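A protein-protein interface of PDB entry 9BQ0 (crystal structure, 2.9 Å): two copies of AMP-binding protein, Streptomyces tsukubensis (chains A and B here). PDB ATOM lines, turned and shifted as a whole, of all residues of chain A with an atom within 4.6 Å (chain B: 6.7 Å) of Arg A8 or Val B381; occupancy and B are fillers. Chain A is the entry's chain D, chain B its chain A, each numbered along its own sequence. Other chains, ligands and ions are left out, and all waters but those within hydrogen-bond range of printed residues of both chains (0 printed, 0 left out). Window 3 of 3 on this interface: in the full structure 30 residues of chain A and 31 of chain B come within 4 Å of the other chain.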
ATOM      1  N   MET A   2       1.168  23.014  12.446  1.00  0.00           N
ATOM      2  CA  MET A   2       0.670  23.206  13.829  1.00  0.00           C
ATOM      3  C   MET A   2      -0.820  23.490  13.721  1.00  0.00           C
ATOM      4  O   MET A   2      -1.235  23.963  12.658  1.00  0.00           O
ATOM      5  CB  MET A   2       1.370  24.390  14.496  1.00  0.00           C
ATOM      6  CG  MET A   2       0.733  24.843  15.788  1.00  0.00           C
ATOM      7  SD  MET A   2       1.752  26.059  16.660  1.00  0.00           S
ATOM      8  CE  MET A   2       1.486  27.501  15.633  1.00  0.00           C
ATOM      9  N   ILE A   3      -1.606  23.205  14.751  1.00  0.00           N
ATOM     10  CA  ILE A   3      -3.060  23.392  14.636  1.00  0.00           C
ATOM     11  C   ILE A   3      -3.362  24.883  14.431  1.00  0.00           C
ATOM     12  O   ILE A   3      -2.525  25.751  14.664  1.00  0.00           O
ATOM     13  CB  ILE A   3      -3.798  22.820  15.852  1.00  0.00           C
ATOM     14  CG1 ILE A   3      -3.176  23.372  17.120  1.00  0.00           C
ATOM     15  CG2 ILE A   3      -3.697  21.270  15.851  1.00  0.00           C
ATOM     16  CD1 ILE A   3      -4.162  23.662  18.185  1.00  0.00           C
ATOM     17  N   SER A   4      -4.538  25.170  13.904  1.00  0.00           N
ATOM     18  CA  SER A   4      -4.884  26.568  13.686  1.00  0.00           C
ATOM     19  C   SER A   4      -5.005  27.323  15.007  1.00  0.00           C
ATOM     20  O   SER A   4      -5.115  26.736  16.092  1.00  0.00           O
ATOM     21  CB  SER A   4      -6.205  26.692  12.925  1.00  0.00           C
ATOM     22  OG  SER A   4      -7.169  25.780  13.434  1.00  0.00           O
ATOM     23  N   GLU A   5      -4.983  28.657  14.907  1.00  0.00           N
ATOM     24  CA  GLU A   5      -5.416  29.442  16.052  1.00  0.00           C
ATOM     25  C   GLU A   5      -6.831  29.064  16.416  1.00  0.00           C
ATOM     26  O   GLU A   5      -7.239  29.232  17.562  1.00  0.00           O
ATOM     27  CB  GLU A   5      -5.382  30.942  15.795  1.00  0.00           C
ATOM     28  CG  GLU A   5      -5.823  31.754  17.025  1.00  0.00           C
ATOM     29  CD  GLU A   5      -4.750  31.900  18.118  1.00  0.00           C
ATOM     30  OE1 GLU A   5      -3.572  31.525  17.912  1.00  0.00           O
ATOM     31  OE2 GLU A   5      -5.071  32.409  19.206  1.00  0.00           O
ATOM     32  N   ASP A   6      -7.614  28.587  15.454  1.00  0.00           N
ATOM     33  CA  ASP A   6      -9.009  28.321  15.760  1.00  0.00           C
ATOM     34  C   ASP A   6      -9.172  27.102  16.654  1.00  0.00           C
ATOM     35  O   ASP A   6      -9.975  27.115  17.592  1.00  0.00           O
ATOM     36  CB  ASP A   6      -9.813  28.134  14.482  1.00  0.00           C
ATOM     37  CG  ASP A   6     -11.300  28.213  14.729  1.00  0.00           C
ATOM     38  OD1 ASP A   6     -11.803  29.300  15.094  1.00  0.00           O
ATOM     39  OD2 ASP A   6     -11.966  27.169  14.605  1.00  0.00           O
ATOM     40  N   LEU A   7      -8.442  26.029  16.384  1.00  0.00           N
ATOM     41  CA  LEU A   7      -8.605  24.823  17.196  1.00  0.00           C
ATOM     42  C   LEU A   7      -7.983  25.016  18.584  1.00  0.00           C
ATOM     43  O   LEU A   7      -8.566  24.598  19.605  1.00  0.00           O
ATOM     44  CB  LEU A   7      -8.010  23.629  16.436  1.00  0.00           C
ATOM     45  CG  LEU A   7      -7.917  22.349  17.237  1.00  0.00           C
ATOM     46  CD1 LEU A   7      -9.324  21.889  17.468  1.00  0.00           C
ATOM     47  CD2 LEU A   7      -7.102  21.311  16.560  1.00  0.00           C
ATOM     48  N   ARG A   8      -6.777  25.614  18.626  1.00  0.00           N
ATOM     49  CA  ARG A   8      -6.120  25.911  19.894  1.00  0.00           C
ATOM     50  C   ARG A   8      -7.067  26.628  20.846  1.00  0.00           C
ATOM     51  O   ARG A   8      -7.282  26.195  21.989  1.00  0.00           O
ATOM     52  CB  ARG A   8      -4.880  26.757  19.627  1.00  0.00           C
ATOM     53  CG  ARG A   8      -4.432  27.662  20.752  1.00  0.00           C
ATOM     54  CD  ARG A   8      -3.234  28.489  20.306  1.00  0.00           C
ATOM     55  NE  ARG A   8      -2.566  29.178  21.396  1.00  0.00           N
ATOM     56  CZ  ARG A   8      -1.751  28.598  22.266  1.00  0.00           C
ATOM     57  NH1 ARG A   8      -1.379  27.330  22.141  1.00  0.00           N
ATOM     58  NH2 ARG A   8      -1.320  29.302  23.308  1.00  0.00           N
ATOM     59  N   GLN A   9      -7.655  27.731  20.382  1.00  0.00           N
ATOM     60  CA  GLN A   9      -8.524  28.486  21.269  1.00  0.00           C
ATOM     61  C   GLN A   9      -9.720  27.626  21.676  1.00  0.00           C
ATOM     62  O   GLN A   9     -10.115  27.605  22.851  1.00  0.00           O
ATOM     63  CB  GLN A   9      -8.946  29.803  20.608  1.00  0.00           C
ATOM     64  CG  GLN A   9      -7.771  30.739  20.332  1.00  0.00           C
ATOM     65  CD  GLN A   9      -7.053  31.186  21.584  1.00  0.00           C
ATOM     66  OE1 GLN A   9      -5.825  31.232  21.643  1.00  0.00           O
ATOM     67  NE2 GLN A   9      -7.826  31.500  22.610  1.00  0.00           N
ATOM     68  N   LYS A  10     -10.274  26.862  20.753  1.00  0.00           N
ATOM     69  CA  LYS A  10     -11.426  25.993  21.063  1.00  0.00           C
ATOM     70  C   LYS A  10     -11.001  24.997  22.135  1.00  0.00           C
ATOM     71  O   LYS A  10     -11.793  24.782  23.052  1.00  0.00           O
ATOM     72  CB  LYS A  10     -11.910  25.293  19.797  1.00  0.00           C
ATOM     73  CG  LYS A  10     -12.936  26.059  18.985  1.00  0.00           C
ATOM     74  CD  LYS A  10     -13.676  25.174  18.022  1.00  0.00           C
ATOM     75  CE  LYS A  10     -13.748  25.761  16.631  1.00  0.00           C
ATOM     76  NZ  LYS A  10     -15.141  25.781  16.134  1.00  0.00           N
ATOM     77  N   VAL A  11      -9.810  24.412  22.022  1.00  0.00           N
ATOM     78  CA  VAL A  11      -9.324  23.417  22.963  1.00  0.00           C
ATOM     79  C   VAL A  11      -9.068  24.044  24.332  1.00  0.00           C
ATOM     80  O   VAL A  11      -9.483  23.509  25.373  1.00  0.00           O
ATOM     81  CB  VAL A  11      -8.057  22.767  22.386  1.00  0.00           C
ATOM     82  CG1 VAL A  11      -7.303  21.988  23.435  1.00  0.00           C
ATOM     83  CG2 VAL A  11      -8.446  21.885  21.205  1.00  0.00           C
ATOM     84  N   LEU A  12      -8.336  25.164  24.350  1.00  0.00           N
ATOM     85  CA  LEU A  12      -7.972  25.816  25.591  1.00  0.00           C
ATOM     86  C   LEU A  12      -9.173  26.489  26.275  1.00  0.00           C
ATOM     87  O   LEU A  12      -9.109  26.839  27.461  1.00  0.00           O
ATOM     88  CB  LEU A  12      -6.891  26.824  25.277  1.00  0.00           C
ATOM     89  CG  LEU A  12      -5.494  26.453  24.855  1.00  0.00           C
ATOM     90  CD1 LEU A  12      -4.701  27.743  24.563  1.00  0.00           C
ATOM     91  CD2 LEU A  12      -4.872  25.579  25.920  1.00  0.00           C
ATOM     92  N   LEU A 211       0.283  21.950  24.502  1.00  0.00           N
ATOM     93  CA  LEU A 211      -0.528  22.653  23.483  1.00  0.00           C
ATOM     94  C   LEU A 211      -0.524  24.134  23.834  1.00  0.00           C
ATOM     95  O   LEU A 211      -0.404  24.909  22.909  1.00  0.00           O
ATOM     96  CB  LEU A 211      -1.959  22.112  23.437  1.00  0.00           C
ATOM     97  CG  LEU A 211      -2.821  22.646  22.296  1.00  0.00           C
ATOM     98  CD1 LEU A 211      -3.686  21.549  21.717  1.00  0.00           C
ATOM     99  CD2 LEU A 211      -3.683  23.808  22.757  1.00  0.00           C
ATOM    100  N   ALA A 212      -0.633  24.488  25.111  1.00  0.00           N
ATOM    101  CA  ALA A 212      -0.708  25.880  25.600  1.00  0.00           C
ATOM    102  C   ALA A 212       0.596  26.619  25.395  1.00  0.00           C
ATOM    103  O   ALA A 212       0.541  27.810  25.165  1.00  0.00           O
ATOM    104  CB  ALA A 212      -1.052  25.843  27.047  1.00  0.00           C
ATOM    105  N   GLY A 214       2.401  26.150  22.928  1.00  0.00           N
ATOM    106  CA  GLY A 214       2.719  26.088  21.519  1.00  0.00           C
ATOM    107  C   GLY A 214       3.582  24.906  21.106  1.00  0.00           C
ATOM    108  O   GLY A 214       4.421  25.067  20.203  1.00  0.00           O
ATOM    109  N   ALA B 372       6.371  31.785  27.444  1.00  0.00           N
ATOM    110  CA  ALA B 372       6.886  32.602  26.348  1.00  0.00           C
ATOM    111  C   ALA B 372       6.316  32.135  25.027  1.00  0.00           C
ATOM    112  O   ALA B 372       6.008  30.952  24.836  1.00  0.00           O
ATOM    113  CB  ALA B 372       8.421  32.565  26.262  1.00  0.00           C
ATOM    114  N   ALA B 373       6.180  33.095  24.122  1.00  0.00           N
ATOM    115  CA  ALA B 373       5.549  32.890  22.832  1.00  0.00           C
ATOM    116  C   ALA B 373       6.075  33.900  21.818  1.00  0.00           C
ATOM    117  O   ALA B 373       6.430  35.038  22.154  1.00  0.00           O
ATOM    118  CB  ALA B 373       4.019  33.007  22.963  1.00  0.00           C
ATOM    119  N   VAL B 374       6.140  33.456  20.572  1.00  0.00           N
ATOM    120  CA  VAL B 374       6.325  34.338  19.431  1.00  0.00           C
ATOM    121  C   VAL B 374       4.938  34.590  18.862  1.00  0.00           C
ATOM    122  O   VAL B 374       4.220  33.650  18.506  1.00  0.00           O
ATOM    123  CB  VAL B 374       7.277  33.736  18.394  1.00  0.00           C
ATOM    124  CG1 VAL B 374       7.153  34.528  17.138  1.00  0.00           C
ATOM    125  CG2 VAL B 374       8.729  33.726  18.914  1.00  0.00           C
ATOM    126  N   VAL B 375       4.513  35.835  18.886  1.00  0.00           N
ATOM    127  CA  VAL B 375       3.112  36.183  18.671  1.00  0.00           C
ATOM    128  C   VAL B 375       2.940  36.903  17.349  1.00  0.00           C
ATOM    129  O   VAL B 375       3.802  37.682  16.936  1.00  0.00           O
ATOM    130  CB  VAL B 375       2.622  37.006  19.890  1.00  0.00           C
ATOM    131  CG1 VAL B 375       1.889  38.247  19.518  1.00  0.00           C
ATOM    132  CG2 VAL B 375       1.790  36.110  20.785  1.00  0.00           C
ATOM    133  N   GLY B 376       1.783  36.678  16.707  1.00  0.00           N
ATOM    134  CA  GLY B 376       1.469  37.414  15.500  1.00  0.00           C
ATOM    135  C   GLY B 376       0.926  38.816  15.795  1.00  0.00           C
ATOM    136  O   GLY B 376       0.856  39.291  16.924  1.00  0.00           O
ATOM    137  N   ASP B 378      -2.111  39.781  15.467  1.00  0.00           N
ATOM    138  CA  ASP B 378      -3.349  39.592  16.217  1.00  0.00           C
ATOM    139  C   ASP B 378      -3.130  38.929  17.565  1.00  0.00           C
ATOM    140  O   ASP B 378      -4.108  38.691  18.285  1.00  0.00           O
ATOM    141  CB  ASP B 378      -4.296  38.716  15.432  1.00  0.00           C
ATOM    142  CG  ASP B 378      -3.791  37.329  15.359  1.00  0.00           C
ATOM    143  OD1 ASP B 378      -2.558  37.186  15.274  1.00  0.00           O
ATOM    144  OD2 ASP B 378      -4.595  36.387  15.361  1.00  0.00           O
ATOM    145  N   GLY B 379      -1.898  38.591  17.926  1.00  0.00           N
ATOM    146  CA  GLY B 379      -1.601  37.958  19.221  1.00  0.00           C
ATOM    147  C   GLY B 379      -1.715  36.457  19.153  1.00  0.00           C
ATOM    148  O   GLY B 379      -1.818  35.839  20.213  1.00  0.00           O
ATOM    149  N   SER B 380      -1.673  35.884  17.958  1.00  0.00           N
ATOM    150  CA  SER B 380      -1.807  34.428  17.729  1.00  0.00           C
ATOM    151  C   SER B 380      -0.454  33.739  17.887  1.00  0.00           C
ATOM    152  O   SER B 380       0.461  34.068  17.151  1.00  0.00           O
ATOM    153  CB  SER B 380      -2.381  34.217  16.368  1.00  0.00           C
ATOM    154  OG  SER B 380      -2.177  32.887  15.932  1.00  0.00           O
ATOM    155  N   VAL B 381      -0.330  32.788  18.798  1.00  0.00           N
ATOM    156  CA  VAL B 381       0.937  32.029  18.982  1.00  0.00           C
ATOM    157  C   VAL B 381       1.418  31.581  17.606  1.00  0.00           C
ATOM    158  O   VAL B 381       0.648  30.895  16.932  1.00  0.00           O
ATOM    159  CB  VAL B 381       0.745  30.828  19.925  1.00  0.00           C
ATOM    160  CG1 VAL B 381       1.876  29.823  19.797  1.00  0.00           C
ATOM    161  CG2 VAL B 381       0.584  31.270  21.368  1.00  0.00           C
ATOM    162  N   LEU B 382       2.647  31.936  17.213  1.00  0.00           N
ATOM    163  CA  LEU B 382       3.195  31.544  15.892  1.00  0.00           C
ATOM    164  C   LEU B 382       3.909  30.194  15.933  1.00  0.00           C
ATOM    165  O   LEU B 382       4.383  29.764  16.980  1.00  0.00           O
ATOM    166  CB  LEU B 382       4.193  32.584  15.379  1.00  0.00           C
ATOM    167  CG  LEU B 382       3.653  34.007  15.203  1.00  0.00           C
ATOM    168  CD1 LEU B 382       4.709  34.903  14.571  1.00  0.00           C
ATOM    169  CD2 LEU B 382       2.348  33.960  14.402  1.00  0.00           C
ATOM    170  N   PRO B 383       4.027  29.476  14.830  1.00  0.00           N
ATOM    171  CA  PRO B 383       4.723  28.191  14.883  1.00  0.00           C
ATOM    172  C   PRO B 383       6.213  28.417  14.991  1.00  0.00           C
ATOM    173  O   PRO B 383       6.678  29.552  14.820  1.00  0.00           O
ATOM    174  CB  PRO B 383       4.323  27.514  13.575  1.00  0.00           C
ATOM    175  CG  PRO B 383       3.808  28.644  12.679  1.00  0.00           C
ATOM    176  CD  PRO B 383       3.529  29.825  13.487  1.00  0.00           C
ATOM    177  N   ARG B 393       4.715  35.904  29.934  1.00  0.00           N
ATOM    178  CA  ARG B 393       3.837  35.894  31.099  1.00  0.00           C
ATOM    179  C   ARG B 393       4.600  35.346  32.289  1.00  0.00           C
ATOM    180  O   ARG B 393       5.278  34.326  32.151  1.00  0.00           O
ATOM    181  CB  ARG B 393       2.615  35.010  30.835  1.00  0.00           C
ATOM    182  CG  ARG B 393       1.376  35.813  30.615  1.00  0.00           C
ATOM    183  CD  ARG B 393       0.529  35.236  29.538  1.00  0.00           C
ATOM    184  NE  ARG B 393       0.202  33.845  29.785  1.00  0.00           N
ATOM    185  CZ  ARG B 393      -0.567  33.133  28.979  1.00  0.00           C
ATOM    186  NH1 ARG B 393      -1.072  33.666  27.872  1.00  0.00           N
ATOM    187  NH2 ARG B 393      -0.862  31.873  29.309  1.00  0.00           N
ATOM    188  N   GLY B 414      -2.632  39.550  22.768  1.00  0.00           N
ATOM    189  CA  GLY B 414      -2.938  38.155  22.760  1.00  0.00           C
ATOM    190  C   GLY B 414      -2.839  37.526  24.122  1.00  0.00           C
ATOM    191  O   GLY B 414      -2.654  36.306  24.227  1.00  0.00           O
ATOM    192  N   TYR B 416      -0.235  38.128  26.175  1.00  0.00           N
ATOM    193  CA  TYR B 416       1.184  38.119  26.494  1.00  0.00           C
ATOM    194  C   TYR B 416       1.600  39.560  26.623  1.00  0.00           C
ATOM    195  O   TYR B 416       0.943  40.445  26.066  1.00  0.00           O
ATOM    196  CB  TYR B 416       2.013  37.445  25.415  1.00  0.00           C
ATOM    197  CG  TYR B 416       1.851  35.941  25.372  1.00  0.00           C
ATOM    198  CD1 TYR B 416       2.605  35.102  26.184  1.00  0.00           C
ATOM    199  CD2 TYR B 416       0.930  35.359  24.530  1.00  0.00           C
ATOM    200  CE1 TYR B 416       2.431  33.730  26.128  1.00  0.00           C
ATOM    201  CE2 TYR B 416       0.757  33.993  24.484  1.00  0.00           C
ATOM    202  CZ  TYR B 416       1.487  33.201  25.269  1.00  0.00           C
ATOM    203  OH  TYR B 416       1.258  31.863  25.165  1.00  0.00           O
ATOM    204  N   ARG B 425      11.474  30.981  17.452  1.00  0.00           N
ATOM    205  CA  ARG B 425      11.810  29.901  18.404  1.00  0.00           C
ATOM    206  C   ARG B 425      11.872  28.570  17.674  1.00  0.00           C
ATOM    207  O   ARG B 425      10.988  28.304  16.875  1.00  0.00           O
ATOM    208  CB  ARG B 425      10.790  29.833  19.539  1.00  0.00           C
ATOM    209  CG  ARG B 425       9.335  29.786  19.104  1.00  0.00           C
ATOM    210  CD  ARG B 425       8.544  28.881  20.022  1.00  0.00           C
ATOM    211  NE  ARG B 425       7.210  28.632  19.495  1.00  0.00           N
ATOM    212  CZ  ARG B 425       6.609  27.450  19.414  1.00  0.00           C
ATOM    213  NH1 ARG B 425       7.197  26.342  19.831  1.00  0.00           N
ATOM    214  NH2 ARG B 425       5.393  27.377  18.910  1.00  0.00           N
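The side-chain hydroxyl (OG) of Ser B380 sits at hydrogen-bond distance from the side-chain carboxylate (OE1) of Glu A5, 2.8 Å away. O of Gly A214 is in hydrogen-bond range of NH2 of Arg B425, 2.8 Å away.
O of Val B374 sits at hydrogen-bond distance from N of Leu B382 (2.7 Å). OD1 of Asp B378 sits at hydrogen-bond distance from N of Ser B380. The guanidinium group (NH2) of Arg B425 lies within hydrogen-bond range of the backbone carbonyl oxygen (O) of Leu B382, 3.2 Å away. OE2 of Glu A5 lies close to OE1 of Gln A9 (2.8 Å). O of Leu A211 is in hydrogen-bond range of NH1 of Arg A8, at 2.7 Å. O of Ala A212 lies within hydrogen-bond range of NH2 of Arg A8 (3.0 Å).
Met A2 touches Val B381. Met A2 touches Leu B382. N of Pro B383 touches CE of Met A2, at 3.3 Å. Val B381 touches Glu A5. NH2 of Arg A8 touches CG2 of Val B381, at 3.4 Å.
Of chain A, only Met A2 (3.7 Å), Glu A5 (3.6 Å) and Arg A8 (3.4 Å) come within 4 Å of Val B381. Of the printed residues of chain A, Arg B425 touches Gly A214. Of the printed residues of chain B, Glu A5 touches Ser B380 and Val B381. Of the printed residues of chain A, Leu B382 touches Met A2. Of the printed residues of chain B, Gly A214 touches Arg B425. Printed residues of chain A within 4 Å of Ser B380: Glu A5. The nearest residue of chain B that does not touch Arg A8 is Tyr B416 (4.1 Å). The nearest residue of chain A that does not touch Val B381 is Gly A214 (4.2 Å).
Hydrophobic or aromatic side chains of chain B that line the printed part of chain A: Val B381 and Pro B383. Printed residues of chain A that touch a printed residue of chain B: Met A2, Glu A5, Arg A8 and Gly A214. Among the printed residues, 7 pairs touch across the chains. Among the printed residues, no Asp or Glu carboxylate lies within 4 Å of a Lys or Arg side-chain nitrogen of the other chain.
No position is printed for both chains. Of the 7 pairs that touch across the chains among the printed residues, none has its exchanged pair printed and touching as well.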
